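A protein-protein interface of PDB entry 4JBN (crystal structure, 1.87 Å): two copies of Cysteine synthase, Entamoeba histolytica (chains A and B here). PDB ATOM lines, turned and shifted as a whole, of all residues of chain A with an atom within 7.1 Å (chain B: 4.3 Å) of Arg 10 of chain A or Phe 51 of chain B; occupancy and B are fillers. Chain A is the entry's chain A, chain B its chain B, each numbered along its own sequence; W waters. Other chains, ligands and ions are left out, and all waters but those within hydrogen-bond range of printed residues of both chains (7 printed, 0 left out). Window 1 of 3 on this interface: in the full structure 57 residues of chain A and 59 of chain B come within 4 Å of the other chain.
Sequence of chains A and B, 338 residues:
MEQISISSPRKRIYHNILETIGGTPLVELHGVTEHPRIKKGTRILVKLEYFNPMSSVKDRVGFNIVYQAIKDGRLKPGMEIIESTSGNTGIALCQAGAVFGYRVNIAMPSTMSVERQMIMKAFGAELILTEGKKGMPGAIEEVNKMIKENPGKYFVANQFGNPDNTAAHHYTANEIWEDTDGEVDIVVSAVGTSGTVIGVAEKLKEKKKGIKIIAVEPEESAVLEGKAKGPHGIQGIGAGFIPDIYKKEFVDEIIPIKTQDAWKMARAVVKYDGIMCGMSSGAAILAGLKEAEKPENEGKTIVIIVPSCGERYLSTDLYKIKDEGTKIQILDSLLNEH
Hydrophobic or aromatic side chains of chain B that line the printed part of chain A: Pro 25, Leu 48, Tyr 50, Phe 51 and Pro 53.
Hydrophobic or aromatic side chains of chain A that line the printed part of chain B: Pro 9, Ile 13, Tyr 14, Ile 17, Tyr 50, Phe 51 and Pro 53.
Among the printed residues, 22 pairs touch across the chains.
Water W5 lies within hydrogen-bond range of the side-chain hydroxyl (OH) of Tyr 50 of chain A (2.6 Å) and the backbone carbonyl oxygen (O) of Pro 53 of chain B (3.2 Å).
Water W6 bridges OH of Tyr 50 of chain B (2.6 Å) and O of Pro 53 of chain A (3.3 Å).
Water W4 lies within hydrogen-bond range of O of Arg 12 of chain A (2.7 Å) and OD2 of Asp 179 of chain B (2.8 Å).
Water W7 bridges OG of Ser 7 of chain A (2.8 Å) and NH1 of Arg 10 of chain B (2.9 Å).
Water W2 lies within hydrogen-bond range of the guanidinium group (NH2) of Arg 10 of chain B (2.9 Å) and the guanidinium group (NH2) of Arg 10 of chain A (3.0 Å).
Water W3 lies within hydrogen-bond range of the guanidinium group of Arg 10 of chain B (2.9 Å), the guanidinium group of Arg 10 of chain A (3.0 Å) and the backbone carbonyl oxygen of Phe 51 of chain B (3.4 Å).
Printed residues of chain B within 4 Å of Pro 9 of chain A: Asp 179 (3.7 Å).
Of chain B, only Arg 10 (3.5 Å), Gly 23 (2.7 Å), Thr 24 (3.8 Å), Pro 25 (3.5 Å), Phe 51 (3.6 Å) and Asp 179 (3.5 Å) come within 4 Å of Arg 10 of chain A.
Printed residues of chain A within 4 Å of Tyr 50 of chain B: Pro 53.
Phe 51 of chain B touches just these residues of chain A: Arg 10, Thr 20, Phe 51 and Pro 53.
The nearest printed residue of chain B that does not touch Arg 10 of chain A is Leu 48 of chain B (7.2 Å).
Among the printed residues, pairs that only touch across the chains: Ser 7 of chain A with Gly 23 of chain B (3.7 Å), Ser 8 of chain A with Gly 23 of chain B (3.4 Å), Pro 9 of chain A with Asp 179 of chain B (3.7 Å), Arg 10 of chain A with Thr 24 of chain B (3.8 Å), Arg 10 of chain A with Pro 25 of chain B (3.5 Å), Arg 10 of chain A with Phe 51 of chain B (3.6 Å), Arg 10 of chain A with Asp 179 of chain B (3.5 Å), Arg 12 of chain A with Asp 179 of chain B (3.7 Å), Ile 13 of chain A with Asp 179 of chain B (3.2 Å), Tyr 14 of chain A with Pro 25 of chain B (3.6 Å), Ile 17 of chain A with Leu 48 of chain B (3.3 Å), Thr 20 of chain A with Phe 51 of chain B (3.3 Å), Tyr 50 of chain A with Pro 53 of chain B (3.8 Å), Phe 51 of chain A with Arg 10 of chain B (3.7 Å), Phe 51 of chain A with Phe 51 of chain B (3.4 Å), Phe 51 of chain A with Pro 53 of chain B (3.7 Å), Pro 53 of chain A with Tyr 50 of chain B (3.9 Å) and Pro 53 of chain A with Phe 51 of chain B (3.8 Å).
The side-chain hydroxyl of Tyr 14 of chain A sits at hydrogen-bond distance from the guanidinium group of Arg 10 of chain A.
The guanidinium group (NH2) of Arg 12 of chain A lies within salt-bridge range of the side-chain carboxylate (OE1) of Glu 19 of chain A (3.2 Å).
The backbone carbonyl oxygen of Ile 17 of chain A is in hydrogen-bond range of the side-chain hydroxyl of Thr 20 of chain A (2.6 Å).
OG1 of Thr 24 of chain B is in hydrogen-bond range of OE2 of Glu 49 of chain B, at 2.6 Å.
The backbone NH of Leu 48 of chain B lies within hydrogen-bond range of the backbone carbonyl oxygen of Pro 25 of chain B, 3.0 Å away.
The backbone carbonyl oxygen of Gly 23 of chain B sits at hydrogen-bond distance from the guanidinium group of Arg 10 of chain A (2.7 Å).
The backbone NH (N) of Lys 11 of chain A sits at hydrogen-bond distance from the side-chain carboxylate (OD1) of Asp 179 of chain B.
The guanidinium group (NE) of Arg 10 of chain B lies within hydrogen-bond range of the backbone carbonyl oxygen (O) of Gly 23 of chain A, 2.8 Å away.
The guanidinium group (NH2) of Arg 10 of chain B sits close to the guanidinium group (NH2) of Arg 10 of chain A (3.5 Å).
Arg 10 of chain A touches Gly 23 of chain B, and with the chains exchanged Gly 23 of chain A touches Arg 10 of chain B.
Arg 10 of chain A touches Phe 51 of chain B, and with the chains exchanged Phe 51 of chain A touches Arg 10 of chain B.
Tyr 50 of chain A touches Pro 53 of chain B, and with the chains exchanged Pro 53 of chain A touches Tyr 50 of chain B.
Phe 51 of chain A touches Pro 53 of chain B, and with the chains exchanged Pro 53 of chain A touches Phe 51 of chain B.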
ATOM      1  N   SER A   7     -38.358  -7.534 -11.637  1.00  0.00           N
ATOM      2  CA  SER A   7     -37.013  -7.234 -12.241  1.00  0.00           C
ATOM      3  C   SER A   7     -37.039  -7.232 -13.729  1.00  0.00           C
ATOM      4  O   SER A   7     -37.771  -8.012 -14.341  1.00  0.00           O
ATOM      5  CB  SER A   7     -35.937  -8.220 -11.764  1.00  0.00           C
ATOM      6  OG  SER A   7     -35.889  -8.120 -10.325  1.00  0.00           O
ATOM      7  N   SER A   8     -36.203  -6.367 -14.318  1.00  0.00           N
ATOM      8  CA  SER A   8     -36.062  -6.243 -15.747  1.00  0.00           C
ATOM      9  C   SER A   8     -35.084  -7.312 -16.250  1.00  0.00           C
ATOM     10  O   SER A   8     -34.341  -7.883 -15.445  1.00  0.00           O
ATOM     11  CB  SER A   8     -35.346  -4.890 -16.063  1.00  0.00           C
ATOM     12  OG  SER A   8     -36.285  -3.878 -15.781  1.00  0.00           O
ATOM     13  N   PRO A   9     -35.052  -7.499 -17.557  1.00  0.00           N
ATOM     14  CA  PRO A   9     -34.156  -8.478 -18.200  1.00  0.00           C
ATOM     15  C   PRO A   9     -32.723  -8.167 -17.825  1.00  0.00           C
ATOM     16  O   PRO A   9     -32.362  -6.960 -17.682  1.00  0.00           O
ATOM     17  CB  PRO A   9     -34.396  -8.239 -19.685  1.00  0.00           C
ATOM     18  CG  PRO A   9     -35.873  -7.841 -19.746  1.00  0.00           C
ATOM     19  CD  PRO A   9     -35.996  -6.906 -18.537  1.00  0.00           C
ATOM     20  N   ARG A  10     -31.892  -9.205 -17.674  1.00  0.00           N
ATOM     21  CA  ARG A  10     -30.445  -9.007 -17.359  1.00  0.00           C
ATOM     22  C   ARG A  10     -29.634  -8.414 -18.553  1.00  0.00           C
ATOM     23  O   ARG A  10     -28.596  -7.760 -18.351  1.00  0.00           O
ATOM     24  CB  ARG A  10     -29.805 -10.331 -16.898  1.00  0.00           C
ATOM     25  CG  ARG A  10     -30.279 -10.705 -15.444  1.00  0.00           C
ATOM     26  CD  ARG A  10     -30.090 -12.221 -15.178  1.00  0.00           C
ATOM     27  NE  ARG A  10     -30.399 -12.471 -13.761  1.00  0.00           N
ATOM     28  CZ  ARG A  10     -29.497 -12.731 -12.825  1.00  0.00           C
ATOM     29  NH1 ARG A  10     -28.213 -12.663 -13.148  1.00  0.00           N
ATOM     30  NH2 ARG A  10     -29.906 -13.022 -11.544  1.00  0.00           N
ATOM     31  N   LYS A  11     -30.149  -8.640 -19.752  1.00  0.00           N
ATOM     32  CA  LYS A  11     -29.519  -8.347 -21.065  1.00  0.00           C
ATOM     33  C   LYS A  11     -28.117  -8.920 -21.126  1.00  0.00           C
ATOM     34  O   LYS A  11     -27.151  -8.191 -21.347  1.00  0.00           O
ATOM     35  CB  LYS A  11     -29.455  -6.836 -21.309  1.00  0.00           C
ATOM     36  CG  LYS A  11     -30.813  -6.182 -21.186  1.00  0.00           C
ATOM     37  CD  LYS A  11     -30.623  -4.722 -20.818  1.00  0.00           C
ATOM     38  CE  LYS A  11     -31.399  -3.871 -21.783  1.00  0.00           C
ATOM     39  NZ  LYS A  11     -30.705  -4.034 -23.090  1.00  0.00           N
ATOM     40  N   ARG A  12     -27.962 -10.193 -20.818  1.00  0.00           N
ATOM     41  CA  ARG A  12     -26.629 -10.818 -20.809  1.00  0.00           C
ATOM     42  C   ARG A  12     -26.994 -12.255 -21.146  1.00  0.00           C
ATOM     43  O   ARG A  12     -28.112 -12.685 -20.764  1.00  0.00           O
ATOM     44  CB  ARG A  12     -25.887 -10.728 -19.411  1.00  0.00           C
ATOM     45  CG  ARG A  12     -24.410 -11.341 -19.414  1.00  0.00           C
ATOM     46  CD  ARG A  12     -23.439 -10.931 -18.268  1.00  0.00           C
ATOM     47  NE  ARG A  12     -22.156 -11.676 -18.303  1.00  0.00           N
ATOM     48  CZ  ARG A  12     -21.330 -11.933 -17.277  1.00  0.00           C
ATOM     49  NH1 ARG A  12     -21.596 -11.606 -15.966  1.00  0.00           N
ATOM     50  NH2 ARG A  12     -20.208 -12.592 -17.549  1.00  0.00           N
ATOM     51  N   ILE A  13     -26.116 -12.975 -21.816  1.00  0.00           N
ATOM     52  CA  ILE A  13     -26.153 -14.413 -21.887  1.00  0.00           C
ATOM     53  C   ILE A  13     -24.891 -14.898 -21.211  1.00  0.00           C
ATOM     54  O   ILE A  13     -23.823 -14.551 -21.604  1.00  0.00           O
ATOM     55  CB  ILE A  13     -26.224 -14.909 -23.327  1.00  0.00           C
ATOM     56  CG1 ILE A  13     -27.597 -14.614 -23.900  1.00  0.00           C
ATOM     57  CG2 ILE A  13     -25.944 -16.377 -23.401  1.00  0.00           C
ATOM     58  CD1 ILE A  13     -27.798 -15.160 -25.270  1.00  0.00           C
ATOM     59  N   TYR A  14     -25.060 -15.666 -20.155  1.00  0.00           N
ATOM     60  CA  TYR A  14     -23.980 -16.124 -19.321  1.00  0.00           C
ATOM     61  C   TYR A  14     -23.280 -17.323 -19.954  1.00  0.00           C
ATOM     62  O   TYR A  14     -23.922 -18.208 -20.418  1.00  0.00           O
ATOM     63  CB  TYR A  14     -24.489 -16.425 -17.909  1.00  0.00           C
ATOM     64  CG  TYR A  14     -25.122 -15.216 -17.268  1.00  0.00           C
ATOM     65  CD1 TYR A  14     -24.387 -14.379 -16.506  1.00  0.00           C
ATOM     66  CD2 TYR A  14     -26.418 -14.892 -17.494  1.00  0.00           C
ATOM     67  CE1 TYR A  14     -24.934 -13.268 -15.932  1.00  0.00           C
ATOM     68  CE2 TYR A  14     -26.966 -13.762 -16.960  1.00  0.00           C
ATOM     69  CZ  TYR A  14     -26.207 -12.950 -16.172  1.00  0.00           C
ATOM     70  OH  TYR A  14     -26.696 -11.835 -15.622  1.00  0.00           O
ATOM     71  N   ILE A  17     -22.503 -21.297 -15.512  1.00  0.00           N
ATOM     72  CA  ILE A  17     -23.201 -20.976 -14.263  1.00  0.00           C
ATOM     73  C   ILE A  17     -22.380 -20.073 -13.326  1.00  0.00           C
ATOM     74  O   ILE A  17     -22.948 -19.371 -12.467  1.00  0.00           O
ATOM     75  CB  ILE A  17     -23.694 -22.302 -13.555  1.00  0.00           C
ATOM     76  CG1 ILE A  17     -24.732 -22.061 -12.456  1.00  0.00           C
ATOM     77  CG2 ILE A  17     -22.542 -23.114 -12.997  1.00  0.00           C
ATOM     78  CD1 ILE A  17     -26.104 -21.551 -12.935  1.00  0.00           C
ATOM     79  N   GLU A  19     -20.724 -17.492 -14.071  1.00  0.00           N
ATOM     80  CA  GLU A  19     -20.917 -16.113 -14.350  1.00  0.00           C
ATOM     81  C   GLU A  19     -22.178 -15.504 -13.717  1.00  0.00           C
ATOM     82  O   GLU A  19     -22.320 -14.261 -13.754  1.00  0.00           O
ATOM     83  CB  GLU A  19     -20.954 -15.865 -15.853  1.00  0.00           C
ATOM     84  CG  GLU A  19     -19.635 -16.269 -16.456  1.00  0.00           C
ATOM     85  CD  GLU A  19     -19.471 -15.710 -17.854  1.00  0.00           C
ATOM     86  OE1 GLU A  19     -20.426 -15.585 -18.629  1.00  0.00           O
ATOM     87  OE2 GLU A  19     -18.316 -15.343 -18.130  1.00  0.00           O
ATOM     88  N   THR A  20     -23.048 -16.350 -13.179  1.00  0.00           N
ATOM     89  CA  THR A  20     -24.290 -15.880 -12.492  1.00  0.00           C
ATOM     90  C   THR A  20     -24.016 -15.711 -11.030  1.00  0.00           C
ATOM     91  O   THR A  20     -24.892 -15.260 -10.316  1.00  0.00           O
ATOM     92  CB  THR A  20     -25.488 -16.894 -12.634  1.00  0.00           C
ATOM     93  OG1 THR A  20     -25.183 -18.083 -11.878  1.00  0.00           O
ATOM     94  CG2 THR A  20     -25.680 -17.255 -14.173  1.00  0.00           C
ATOM     95  N   ILE A  21     -22.789 -15.990 -10.565  1.00  0.00           N
ATOM     96  CA  ILE A  21     -22.418 -15.751  -9.177  1.00  0.00           C
ATOM     97  C   ILE A  21     -22.364 -14.271  -8.928  1.00  0.00           C
ATOM     98  O   ILE A  21     -21.939 -13.540  -9.785  1.00  0.00           O
ATOM     99  CB  ILE A  21     -21.067 -16.483  -8.804  1.00  0.00           C
ATOM    100  CG1 ILE A  21     -21.304 -18.016  -8.676  1.00  0.00           C
ATOM    101  CG2 ILE A  21     -20.473 -15.973  -7.475  1.00  0.00           C
ATOM    102  CD1 ILE A  21     -20.021 -18.849  -8.791  1.00  0.00           C
ATOM    103  N   GLY A  22     -22.798 -13.855  -7.763  1.00  0.00           N
ATOM    104  CA  GLY A  22     -22.636 -12.415  -7.360  1.00  0.00           C
ATOM    105  C   GLY A  22     -23.748 -11.511  -7.845  1.00  0.00           C
ATOM    106  O   GLY A  22     -24.780 -11.996  -8.353  1.00  0.00           O
ATOM    107  N   GLY A  23     -23.545 -10.188  -7.717  1.00  0.00           N
ATOM    108  CA  GLY A  23     -24.588  -9.186  -8.124  1.00  0.00           C
ATOM    109  C   GLY A  23     -25.904  -9.525  -7.416  1.00  0.00           C
ATOM    110  O   GLY A  23     -26.954  -9.536  -8.094  1.00  0.00           O
ATOM    111  N   TYR A  50     -28.396 -15.827  -1.060  1.00  0.00           N
ATOM    112  CA  TYR A  50     -28.957 -17.110  -1.554  1.00  0.00           C
ATOM    113  C   TYR A  50     -29.484 -16.918  -2.973  1.00  0.00           C
ATOM    114  O   TYR A  50     -29.959 -17.860  -3.589  1.00  0.00           O
ATOM    115  CB  TYR A  50     -30.023 -17.650  -0.590  1.00  0.00           C
ATOM    116  CG  TYR A  50     -31.196 -16.770  -0.331  1.00  0.00           C
ATOM    117  CD1 TYR A  50     -32.228 -16.626  -1.283  1.00  0.00           C
ATOM    118  CD2 TYR A  50     -31.375 -16.203   0.932  1.00  0.00           C
ATOM    119  CE1 TYR A  50     -33.341 -15.806  -0.977  1.00  0.00           C
ATOM    120  CE2 TYR A  50     -32.481 -15.451   1.249  1.00  0.00           C
ATOM    121  CZ  TYR A  50     -33.472 -15.261   0.293  1.00  0.00           C
ATOM    122  OH  TYR A  50     -34.580 -14.540   0.655  1.00  0.00           O
ATOM    123  N   PHE A  51     -29.362 -15.711  -3.516  1.00  0.00           N
ATOM    124  CA  PHE A  51     -29.573 -15.582  -4.977  1.00  0.00           C
ATOM    125  C   PHE A  51     -28.446 -16.168  -5.847  1.00  0.00           C
ATOM    126  O   PHE A  51     -28.637 -16.385  -7.035  1.00  0.00           O
ATOM    127  CB  PHE A  51     -29.843 -14.140  -5.403  1.00  0.00           C
ATOM    128  CG  PHE A  51     -31.278 -13.739  -5.198  1.00  0.00           C
ATOM    129  CD1 PHE A  51     -31.809 -13.670  -3.902  1.00  0.00           C
ATOM    130  CD2 PHE A  51     -32.059 -13.426  -6.307  1.00  0.00           C
ATOM    131  CE1 PHE A  51     -33.142 -13.344  -3.727  1.00  0.00           C
ATOM    132  CE2 PHE A  51     -33.386 -13.025  -6.144  1.00  0.00           C
ATOM    133  CZ  PHE A  51     -33.903 -13.006  -4.861  1.00  0.00           C
ATOM    134  N   ASN A  52     -27.286 -16.413  -5.258  1.00  0.00           N
ATOM    135  CA  ASN A  52     -26.239 -17.208  -5.932  1.00  0.00           C
ATOM    136  C   ASN A  52     -26.757 -18.559  -6.481  1.00  0.00           C
ATOM    137  O   ASN A  52     -27.732 -19.081  -6.007  1.00  0.00           O
ATOM    138  CB  ASN A  52     -25.082 -17.443  -4.959  1.00  0.00           C
ATOM    139  CG  ASN A  52     -24.221 -16.213  -4.781  1.00  0.00           C
ATOM    140  OD1 ASN A  52     -24.021 -15.698  -3.642  1.00  0.00           O
ATOM    141  ND2 ASN A  52     -23.754 -15.695  -5.883  1.00  0.00           N
ATOM    142  N   PRO A  53     -26.100 -19.114  -7.481  1.00  0.00           N
ATOM    143  CA  PRO A  53     -26.635 -20.313  -8.118  1.00  0.00           C
ATOM    144  C   PRO A  53     -26.812 -21.490  -7.204  1.00  0.00           C
ATOM    145  O   PRO A  53     -27.708 -22.215  -7.450  1.00  0.00           O
ATOM    146  CB  PRO A  53     -25.645 -20.620  -9.230  1.00  0.00           C
ATOM    147  CG  PRO A  53     -24.500 -19.754  -9.009  1.00  0.00           C
ATOM    148  CD  PRO A  53     -24.946 -18.594  -8.198  1.00  0.00           C
ATOM    149  N   MET A  54     -25.985 -21.710  -6.211  1.00  0.00           N
ATOM    150  CA  MET A  54     -26.281 -22.774  -5.294  1.00  0.00           C
ATOM    151  C   MET A  54     -26.793 -22.228  -3.944  1.00  0.00           C
ATOM    152  O   MET A  54     -26.672 -22.856  -2.958  1.00  0.00           O
ATOM    153  CB  MET A  54     -25.127 -23.778  -5.167  1.00  0.00           C
ATOM    154  CG  MET A  54     -25.032 -24.755  -6.327  1.00  0.00           C
ATOM    155  SD  MET A  54     -26.489 -25.785  -6.509  1.00  0.00           S
ATOM    156  CE  MET A  54     -26.499 -26.636  -4.982  1.00  0.00           C
ATOM    157  N   ASP A  59     -20.791 -19.746  -2.729  1.00  0.00           N
ATOM    158  CA  ASP A  59     -20.595 -19.800  -4.173  1.00  0.00           C
ATOM    159  C   ASP A  59     -19.452 -18.862  -4.611  1.00  0.00           C
ATOM    160  O   ASP A  59     -18.602 -19.235  -5.461  1.00  0.00           O
ATOM    161  CB  ASP A  59     -21.875 -19.381  -4.947  1.00  0.00           C
ATOM    162  CG  ASP A  59     -22.967 -20.437  -4.859  1.00  0.00           C
ATOM    163  OD1 ASP A  59     -22.811 -21.333  -4.057  1.00  0.00           O
ATOM    164  OD2 ASP A  59     -23.898 -20.413  -5.674  1.00  0.00           O
ATOM    165  N   ARG B  10     -26.515  -5.020  -9.209  1.00  0.00           N
ATOM    166  CA  ARG B  10     -27.833  -4.775  -9.772  1.00  0.00           C
ATOM    167  C   ARG B  10     -28.091  -3.277  -9.908  1.00  0.00           C
ATOM    168  O   ARG B  10     -28.900  -2.884 -10.784  1.00  0.00           O
ATOM    169  CB  ARG B  10     -28.917  -5.442  -8.919  1.00  0.00           C
ATOM    170  CG  ARG B  10     -29.004  -6.963  -9.148  1.00  0.00           C
ATOM    171  CD  ARG B  10     -29.537  -7.648  -7.952  1.00  0.00           C
ATOM    172  NE  ARG B  10     -29.705  -9.107  -8.267  1.00  0.00           N
ATOM    173  CZ  ARG B  10     -30.841  -9.694  -8.619  1.00  0.00           C
ATOM    174  NH1 ARG B  10     -31.932  -8.970  -8.739  1.00  0.00           N
ATOM    175  NH2 ARG B  10     -30.883 -11.016  -8.873  1.00  0.00           N
ATOM    176  N   GLY B  23     -36.531 -11.476 -14.310  1.00  0.00           N
ATOM    177  CA  GLY B  23     -35.188 -11.084 -14.858  1.00  0.00           C
ATOM    178  C   GLY B  23     -34.196 -12.230 -14.527  1.00  0.00           C
ATOM    179  O   GLY B  23     -33.077 -11.991 -14.032  1.00  0.00           O
ATOM    180  N   THR B  24     -34.617 -13.479 -14.812  1.00  0.00           N
ATOM    181  CA  THR B  24     -33.765 -14.614 -14.520  1.00  0.00           C
ATOM    182  C   THR B  24     -32.713 -14.893 -15.605  1.00  0.00           C
ATOM    183  O   THR B  24     -32.846 -14.483 -16.799  1.00  0.00           O
ATOM    184  CB  THR B  24     -34.652 -15.903 -14.388  1.00  0.00           C
ATOM    185  OG1 THR B  24     -35.375 -16.020 -15.596  1.00  0.00           O
ATOM    186  CG2 THR B  24     -35.610 -15.783 -13.184  1.00  0.00           C
ATOM    187  N   PRO B  25     -31.587 -15.528 -15.205  1.00  0.00           N
ATOM    188  CA  PRO B  25     -30.473 -15.544 -16.165  1.00  0.00           C
ATOM    189  C   PRO B  25     -30.606 -16.589 -17.290  1.00  0.00           C
ATOM    190  O   PRO B  25     -31.153 -17.753 -17.083  1.00  0.00           O
ATOM    191  CB  PRO B  25     -29.280 -15.888 -15.283  1.00  0.00           C
ATOM    192  CG  PRO B  25     -29.842 -16.682 -14.104  1.00  0.00           C
ATOM    193  CD  PRO B  25     -31.237 -16.118 -13.895  1.00  0.00           C
ATOM    194  N   LEU B  48     -32.951 -19.966 -16.089  1.00  0.00           N
ATOM    195  CA  LEU B  48     -32.914 -20.619 -14.788  1.00  0.00           C
ATOM    196  C   LEU B  48     -33.907 -19.958 -13.862  1.00  0.00           C
ATOM    197  O   LEU B  48     -33.623 -18.958 -13.195  1.00  0.00           O
ATOM    198  CB  LEU B  48     -31.455 -20.525 -14.206  1.00  0.00           C
ATOM    199  CG  LEU B  48     -30.394 -21.187 -15.098  1.00  0.00           C
ATOM    200  CD1 LEU B  48     -29.041 -21.149 -14.379  1.00  0.00           C
ATOM    201  CD2 LEU B  48     -30.736 -22.636 -15.484  1.00  0.00           C
ATOM    202  N   GLU B  49     -35.103 -20.481 -13.828  1.00  0.00           N
ATOM    203  CA  GLU B  49     -36.182 -19.804 -13.085  1.00  0.00           C
ATOM    204  C   GLU B  49     -36.077 -20.053 -11.617  1.00  0.00           C
ATOM    205  O   GLU B  49     -36.803 -19.422 -10.831  1.00  0.00           O
ATOM    206  CB  GLU B  49     -37.576 -20.300 -13.592  1.00  0.00           C
ATOM    207  CG  GLU B  49     -37.845 -19.786 -15.005  1.00  0.00           C
ATOM    208  CD  GLU B  49     -38.120 -18.288 -14.941  1.00  0.00           C
ATOM    209  OE1 GLU B  49     -38.839 -17.855 -14.029  1.00  0.00           O
ATOM    210  OE2 GLU B  49     -37.524 -17.536 -15.770  1.00  0.00           O
ATOM    211  N   TYR B  50     -35.084 -20.868 -11.189  1.00  0.00           N
ATOM    212  CA  TYR B  50     -34.834 -20.974  -9.743  1.00  0.00           C
ATOM    213  C   TYR B  50     -34.038 -19.788  -9.161  1.00  0.00           C
ATOM    214  O   TYR B  50     -33.795 -19.725  -7.962  1.00  0.00           O
ATOM    215  CB  TYR B  50     -34.192 -22.316  -9.392  1.00  0.00           C
ATOM    216  CG  TYR B  50     -32.870 -22.633 -10.083  1.00  0.00           C
ATOM    217  CD1 TYR B  50     -31.648 -22.158  -9.571  1.00  0.00           C
ATOM    218  CD2 TYR B  50     -32.837 -23.511 -11.171  1.00  0.00           C
ATOM    219  CE1 TYR B  50     -30.448 -22.525 -10.161  1.00  0.00           C
ATOM    220  CE2 TYR B  50     -31.648 -23.896 -11.782  1.00  0.00           C
ATOM    221  CZ  TYR B  50     -30.472 -23.402 -11.223  1.00  0.00           C
ATOM    222  OH  TYR B  50     -29.286 -23.771 -11.756  1.00  0.00           O
ATOM    223  N   PHE B  51     -33.660 -18.813 -10.015  1.00  0.00           N
ATOM    224  CA  PHE B  51     -33.120 -17.555  -9.532  1.00  0.00           C
ATOM    225  C   PHE B  51     -34.195 -16.684  -8.933  1.00  0.00           C
ATOM    226  O   PHE B  51     -33.885 -15.757  -8.211  1.00  0.00           O
ATOM    227  CB  PHE B  51     -32.328 -16.811 -10.645  1.00  0.00           C
ATOM    228  CG  PHE B  51     -30.869 -17.287 -10.677  1.00  0.00           C
ATOM    229  CD1 PHE B  51     -30.607 -18.617 -11.099  1.00  0.00           C
ATOM    230  CD2 PHE B  51     -29.827 -16.430 -10.336  1.00  0.00           C
ATOM    231  CE1 PHE B  51     -29.286 -19.081 -11.178  1.00  0.00           C
ATOM    232  CE2 PHE B  51     -28.501 -16.905 -10.370  1.00  0.00           C
ATOM    233  CZ  PHE B  51     -28.279 -18.227 -10.786  1.00  0.00           C
ATOM    234  N   ASN B  52     -35.462 -17.002  -9.160  1.00  0.00           N
ATOM    235  CA  ASN B  52     -36.561 -16.330  -8.342  1.00  0.00           C
ATOM    236  C   ASN B  52     -36.384 -16.473  -6.820  1.00  0.00           C
ATOM    237  O   ASN B  52     -35.678 -17.414  -6.384  1.00  0.00           O
ATOM    238  CB  ASN B  52     -37.906 -16.957  -8.801  1.00  0.00           C
ATOM    239  CG  ASN B  52     -38.295 -16.414 -10.124  1.00  0.00           C
ATOM    240  OD1 ASN B  52     -38.494 -17.141 -11.124  1.00  0.00           O
ATOM    241  ND2 ASN B  52     -38.395 -15.094 -10.155  1.00  0.00           N
ATOM    242  N   PRO B  53     -36.974 -15.555  -5.988  1.00  0.00           N
ATOM    243  CA  PRO B  53     -36.593 -15.584  -4.519  1.00  0.00           C
ATOM    244  C   PRO B  53     -36.969 -16.871  -3.786  1.00  0.00           C
ATOM    245  O   PRO B  53     -36.307 -17.231  -2.797  1.00  0.00           O
ATOM    246  CB  PRO B  53     -37.361 -14.433  -3.923  1.00  0.00           C
ATOM    247  CG  PRO B  53     -38.427 -13.985  -5.003  1.00  0.00           C
ATOM    248  CD  PRO B  53     -37.706 -14.305  -6.315  1.00  0.00           C
ATOM    249  N   ASP B 179     -32.666 -10.737 -23.911  1.00  0.00           N
ATOM    250  CA  ASP B 179     -31.349 -11.432 -23.584  1.00  0.00           C
ATOM    251  C   ASP B 179     -30.690 -12.035 -24.788  1.00  0.00           C
ATOM    252  O   ASP B 179     -29.411 -12.087 -24.824  1.00  0.00           O
ATOM    253  CB  ASP B 179     -31.440 -12.461 -22.472  1.00  0.00           C
ATOM    254  CG  ASP B 179     -31.793 -11.850 -21.118  1.00  0.00           C
ATOM    255  OD1 ASP B 179     -31.763 -10.592 -20.928  1.00  0.00           O
ATOM    256  OD2 ASP B 179     -32.082 -12.629 -20.168  1.00  0.00           O
HETATM  257  O   HOH W   1     -33.194 -11.763 -17.819  1.00  0.00           O
HETATM  258  O   HOH W   2     -28.765 -12.987  -8.758  1.00  0.00           O
HETATM  259  O   HOH W   3     -32.456 -13.215 -10.014  1.00  0.00           O
HETATM  260  O   HOH W   4     -29.781 -13.488 -18.752  1.00  0.00           O
HETATM  261  O   HOH W   5     -36.755 -15.808   0.004  1.00  0.00           O
HETATM  262  O   HOH W   6     -27.451 -24.251  -9.975  1.00  0.00           O
HETATM  263  O   HOH W   7     -34.246 -10.338  -9.771  1.00  0.00           O
